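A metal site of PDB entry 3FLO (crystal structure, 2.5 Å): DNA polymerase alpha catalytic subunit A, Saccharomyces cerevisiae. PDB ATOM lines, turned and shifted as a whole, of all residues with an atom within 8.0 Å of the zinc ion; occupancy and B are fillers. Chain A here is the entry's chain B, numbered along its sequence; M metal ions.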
ATOM      1  N   GLN A  85     -28.941  -6.592  22.445  1.00  0.00           N
ATOM      2  CA  GLN A  85     -28.069  -5.451  22.249  1.00  0.00           C
ATOM      3  C   GLN A  85     -27.585  -5.353  20.798  1.00  0.00           C
ATOM      4  O   GLN A  85     -27.336  -6.358  20.131  1.00  0.00           O
ATOM      5  CB  GLN A  85     -26.853  -5.543  23.185  1.00  0.00           C
ATOM      6  CG  GLN A  85     -26.098  -4.225  23.210  1.00  0.00           C
ATOM      7  CD  GLN A  85     -25.061  -4.110  24.311  1.00  0.00           C
ATOM      8  OE1 GLN A  85     -24.681  -5.101  24.994  1.00  0.00           O
ATOM      9  NE2 GLN A  85     -24.567  -2.870  24.486  1.00  0.00           N
ATOM     10  N   CYS A  86     -27.417  -4.119  20.332  1.00  0.00           N
ATOM     11  CA  CYS A  86     -26.887  -3.872  19.004  1.00  0.00           C
ATOM     12  C   CYS A  86     -25.344  -3.727  18.965  1.00  0.00           C
ATOM     13  O   CYS A  86     -24.763  -2.941  19.706  1.00  0.00           O
ATOM     14  CB  CYS A  86     -27.501  -2.611  18.461  1.00  0.00           C
ATOM     15  SG  CYS A  86     -26.844  -2.173  16.918  1.00  0.00           S
ATOM     16  N   ASP A  87     -24.736  -4.521  18.079  1.00  0.00           N
ATOM     17  CA  ASP A  87     -23.342  -4.385  17.598  1.00  0.00           C
ATOM     18  C   ASP A  87     -22.770  -3.007  17.372  1.00  0.00           C
ATOM     19  O   ASP A  87     -21.622  -2.783  17.617  1.00  0.00           O
ATOM     20  CB  ASP A  87     -23.261  -4.959  16.163  1.00  0.00           C
ATOM     21  CG  ASP A  87     -22.580  -6.258  16.098  1.00  0.00           C
ATOM     22  OD1 ASP A  87     -22.256  -6.803  17.162  1.00  0.00           O
ATOM     23  OD2 ASP A  87     -22.389  -6.763  14.995  1.00  0.00           O
ATOM     24  N   ASP A  88     -23.528  -2.150  16.737  1.00  0.00           N
ATOM     25  CA  ASP A  88     -22.970  -0.952  16.178  1.00  0.00           C
ATOM     26  C   ASP A  88     -22.635  -0.022  17.343  1.00  0.00           C
ATOM     27  O   ASP A  88     -23.527   0.350  18.122  1.00  0.00           O
ATOM     28  CB  ASP A  88     -23.943  -0.327  15.199  1.00  0.00           C
ATOM     29  CG  ASP A  88     -23.372   0.858  14.528  1.00  0.00           C
ATOM     30  OD1 ASP A  88     -22.212   1.174  14.821  1.00  0.00           O
ATOM     31  OD2 ASP A  88     -24.103   1.461  13.718  1.00  0.00           O
ATOM     32  N   SER A  89     -21.358   0.334  17.447  1.00  0.00           N
ATOM     33  CA  SER A  89     -20.840   1.126  18.573  1.00  0.00           C
ATOM     34  C   SER A  89     -21.483   2.531  18.617  1.00  0.00           C
ATOM     35  O   SER A  89     -21.658   3.093  19.704  1.00  0.00           O
ATOM     36  CB  SER A  89     -19.317   1.259  18.465  1.00  0.00           C
ATOM     37  OG  SER A  89     -18.917   1.747  17.184  1.00  0.00           O
ATOM     38  N   THR A  90     -21.830   3.067  17.437  1.00  0.00           N
ATOM     39  CA  THR A  90     -22.571   4.319  17.330  1.00  0.00           C
ATOM     40  C   THR A  90     -24.104   4.181  17.531  1.00  0.00           C
ATOM     41  O   THR A  90     -24.858   5.035  17.087  1.00  0.00           O
ATOM     42  CB  THR A  90     -22.376   4.909  15.930  1.00  0.00           C
ATOM     43  OG1 THR A  90     -23.305   4.292  15.023  1.00  0.00           O
ATOM     44  CG2 THR A  90     -20.955   4.697  15.423  1.00  0.00           C
ATOM     45  N   CYS A  91     -24.568   3.099  18.144  1.00  0.00           N
ATOM     46  CA  CYS A  91     -26.006   2.877  18.358  1.00  0.00           C
ATOM     47  C   CYS A  91     -26.171   2.223  19.717  1.00  0.00           C
ATOM     48  O   CYS A  91     -26.551   2.891  20.668  1.00  0.00           O
ATOM     49  CB  CYS A  91     -26.572   2.009  17.243  1.00  0.00           C
ATOM     50  SG  CYS A  91     -28.141   1.186  17.617  1.00  0.00           S
ATOM     51  N   GLY A  92     -25.868   0.927  19.801  1.00  0.00           N
ATOM     52  CA  GLY A  92     -25.744   0.224  21.084  1.00  0.00           C
ATOM     53  C   GLY A  92     -27.025  -0.074  21.860  1.00  0.00           C
ATOM     54  O   GLY A  92     -26.962  -0.606  22.973  1.00  0.00           O
ATOM     55  N   ILE A  93     -28.195   0.223  21.275  1.00  0.00           N
ATOM     56  CA  ILE A  93     -29.438   0.158  22.053  1.00  0.00           C
ATOM     57  C   ILE A  93     -29.676  -1.205  22.666  1.00  0.00           C
ATOM     58  O   ILE A  93     -29.271  -2.230  22.146  1.00  0.00           O
ATOM     59  CB  ILE A  93     -30.686   0.658  21.266  1.00  0.00           C
ATOM     60  CG1 ILE A  93     -31.100  -0.294  20.156  1.00  0.00           C
ATOM     61  CG2 ILE A  93     -30.421   2.044  20.694  1.00  0.00           C
ATOM     62  CD1 ILE A  93     -32.465   0.117  19.598  1.00  0.00           C
ATOM     63  N   LYS A 103     -32.195 -10.525  13.831  1.00  0.00           N
ATOM     64  CA  LYS A 103     -30.865  -9.916  13.882  1.00  0.00           C
ATOM     65  C   LYS A 103     -30.908  -8.434  13.531  1.00  0.00           C
ATOM     66  O   LYS A 103     -29.938  -7.723  13.769  1.00  0.00           O
ATOM     67  CB  LYS A 103     -29.905 -10.695  12.941  1.00  0.00           C
ATOM     68  CG  LYS A 103     -29.553 -12.116  13.505  1.00  0.00           C
ATOM     69  CD  LYS A 103     -28.428 -12.858  12.720  1.00  0.00           C
ATOM     70  CE  LYS A 103     -28.009 -14.127  13.509  1.00  0.00           C
ATOM     71  NZ  LYS A 103     -26.602 -14.716  13.196  1.00  0.00           N
ATOM     72  N   ARG A 104     -32.028  -7.980  12.981  1.00  0.00           N
ATOM     73  CA  ARG A 104     -32.141  -6.614  12.500  1.00  0.00           C
ATOM     74  C   ARG A 104     -32.429  -5.608  13.604  1.00  0.00           C
ATOM     75  O   ARG A 104     -33.292  -5.829  14.454  1.00  0.00           O
ATOM     76  CB  ARG A 104     -33.239  -6.512  11.462  1.00  0.00           C
ATOM     77  CG  ARG A 104     -33.330  -5.121  10.916  1.00  0.00           C
ATOM     78  CD  ARG A 104     -34.092  -5.065   9.629  1.00  0.00           C
ATOM     79  NE  ARG A 104     -35.534  -5.102   9.873  1.00  0.00           N
ATOM     80  CZ  ARG A 104     -36.451  -5.197   8.925  1.00  0.00           C
ATOM     81  NH1 ARG A 104     -36.074  -5.287   7.648  1.00  0.00           N
ATOM     82  NH2 ARG A 104     -37.735  -5.213   9.227  1.00  0.00           N
ATOM     83  N   CYS A 105     -31.705  -4.508  13.584  1.00  0.00           N
ATOM     84  CA  CYS A 105     -31.834  -3.464  14.594  1.00  0.00           C
ATOM     85  C   CYS A 105     -33.065  -2.613  14.359  1.00  0.00           C
ATOM     86  O   CYS A 105     -33.368  -2.274  13.246  1.00  0.00           O
ATOM     87  CB  CYS A 105     -30.617  -2.542  14.544  1.00  0.00           C
ATOM     88  SG  CYS A 105     -30.513  -1.390  15.919  1.00  0.00           S
ATOM     89  N   LEU A 106     -33.757  -2.266  15.427  1.00  0.00           N
ATOM     90  CA  LEU A 106     -34.993  -1.493  15.327  1.00  0.00           C
ATOM     91  C   LEU A 106     -34.811   0.022  15.173  1.00  0.00           C
ATOM     92  O   LEU A 106     -35.801   0.694  14.898  1.00  0.00           O
ATOM     93  CB  LEU A 106     -35.909  -1.770  16.515  1.00  0.00           C
ATOM     94  CG  LEU A 106     -36.548  -3.147  16.438  1.00  0.00           C
ATOM     95  CD1 LEU A 106     -37.235  -3.460  17.733  1.00  0.00           C
ATOM     96  CD2 LEU A 106     -37.472  -3.203  15.279  1.00  0.00           C
ATOM     97  N   ASN A 107     -33.590   0.551  15.311  1.00  0.00           N
ATOM     98  CA  ASN A 107     -33.299   1.982  14.925  1.00  0.00           C
ATOM     99  C   ASN A 107     -33.391   2.254  13.433  1.00  0.00           C
ATOM    100  O   ASN A 107     -32.599   1.712  12.652  1.00  0.00           O
ATOM    101  CB  ASN A 107     -31.884   2.439  15.256  1.00  0.00           C
ATOM    102  CG  ASN A 107     -31.774   3.071  16.603  1.00  0.00           C
ATOM    103  OD1 ASN A 107     -32.481   2.681  17.520  1.00  0.00           O
ATOM    104  ND2 ASN A 107     -30.863   4.026  16.750  1.00  0.00           N
ATOM    105  N   ASP A 108     -34.274   3.142  13.029  1.00  0.00           N
ATOM    106  CA  ASP A 108     -34.383   3.456  11.615  1.00  0.00           C
ATOM    107  C   ASP A 108     -32.991   3.429  10.960  1.00  0.00           C
ATOM    108  O   ASP A 108     -32.127   4.250  11.276  1.00  0.00           O
ATOM    109  CB  ASP A 108     -35.048   4.824  11.387  1.00  0.00           C
ATOM    110  CG  ASP A 108     -35.967   4.814  10.180  1.00  0.00           C
ATOM    111  OD1 ASP A 108     -36.781   3.853  10.107  1.00  0.00           O
ATOM    112  OD2 ASP A 108     -35.888   5.733   9.310  1.00  0.00           O
ATOM    113  N   GLY A 109     -32.792   2.455  10.074  1.00  0.00           N
ATOM    114  CA  GLY A 109     -31.639   2.464   9.146  1.00  0.00           C
ATOM    115  C   GLY A 109     -30.332   1.958   9.716  1.00  0.00           C
ATOM    116  O   GLY A 109     -29.306   1.976   9.042  1.00  0.00           O
ATOM    117  N   CYS A 110     -30.344   1.533  10.965  1.00  0.00           N
ATOM    118  CA  CYS A 110     -29.126   1.081  11.586  1.00  0.00           C
ATOM    119  C   CYS A 110     -28.767  -0.305  11.038  1.00  0.00           C
ATOM    120  O   CYS A 110     -29.634  -1.170  10.913  1.00  0.00           O
ATOM    121  CB  CYS A 110     -29.300   1.015  13.094  1.00  0.00           C
ATOM    122  SG  CYS A 110     -27.909   0.284  13.896  1.00  0.00           S
ATOM    123  N   THR A 111     -27.502  -0.514  10.677  1.00  0.00           N
ATOM    124  CA  THR A 111     -27.106  -1.759  10.004  1.00  0.00           C
ATOM    125  C   THR A 111     -26.434  -2.768  10.941  1.00  0.00           C
ATOM    126  O   THR A 111     -25.925  -3.798  10.502  1.00  0.00           O
ATOM    127  CB  THR A 111     -26.167  -1.490   8.855  1.00  0.00           C
ATOM    128  OG1 THR A 111     -24.965  -0.904   9.361  1.00  0.00           O
ATOM    129  CG2 THR A 111     -26.816  -0.545   7.871  1.00  0.00           C
ATOM    130  N   GLY A 112     -26.457  -2.484  12.234  1.00  0.00           N
ATOM    131  CA  GLY A 112     -25.830  -3.343  13.211  1.00  0.00           C
ATOM    132  C   GLY A 112     -26.603  -4.626  13.411  1.00  0.00           C
ATOM    133  O   GLY A 112     -27.758  -4.747  13.008  1.00  0.00           O
ATOM    134  N   VAL A 113     -25.958  -5.601  14.034  1.00  0.00           N
ATOM    135  CA  VAL A 113     -26.585  -6.889  14.279  1.00  0.00           C
ATOM    136  C   VAL A 113     -26.998  -6.997  15.755  1.00  0.00           C
ATOM    137  O   VAL A 113     -26.310  -6.564  16.628  1.00  0.00           O
ATOM    138  CB  VAL A 113     -25.638  -8.028  13.911  1.00  0.00           C
ATOM    139  CG1 VAL A 113     -26.248  -9.389  14.279  1.00  0.00           C
ATOM    140  CG2 VAL A 113     -25.278  -7.942  12.442  1.00  0.00           C
ATOM    141  N   MET A 114     -28.172  -7.553  16.014  1.00  0.00           N
ATOM    142  CA  MET A 114     -28.696  -7.671  17.340  1.00  0.00           C
ATOM    143  C   MET A 114     -28.303  -9.023  17.905  1.00  0.00           C
ATOM    144  O   MET A 114     -28.286 -10.025  17.188  1.00  0.00           O
ATOM    145  CB  MET A 114     -30.216  -7.564  17.314  1.00  0.00           C
ATOM    146  CG  MET A 114     -30.812  -6.217  16.972  1.00  0.00           C
ATOM    147  SD  MET A 114     -30.245  -4.820  17.975  1.00  0.00           S
ATOM    148  CE  MET A 114     -30.798  -5.158  19.674  1.00  0.00           C
HETATM  149 ZN    ZN M   1     -28.334  -0.575  16.059  1.00  0.00          ZN
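The side-chain sulfur (SG) of Cys 105 sits close to the backbone NH (N) of Asn 107 (3.7 Å). The side-chain sulfur of Cys 86 sits close to the backbone NH of Asp 88 (3.3 Å). The backbone carbonyl oxygen (O) of Ile 93 is in hydrogen-bond range of the backbone NH (N) of Cys 86. The backbone NH (N) of Cys 86 sits close to the side-chain sulfur (SD) of Met 114, 3.7 Å away. The side-chain sulfur (SG) of Cys 91 lies close to the backbone NH (N) of Ile 93, at 3.8 Å. The backbone NH of Gly 112 lies close to the side-chain sulfur of Cys 110.
The zinc ion is bound by the side-chain sulfur (SG) of Cys 105 (2.3 Å). The zinc ion is bound by SG of Cys 86, at 2.3 Å. SG of Cys 91 binds the zinc ion, 2.4 Å away. SG of Cys 110 is bound to the zinc ion (2.4 Å). The zinc ion has four donor atoms within binding distance.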
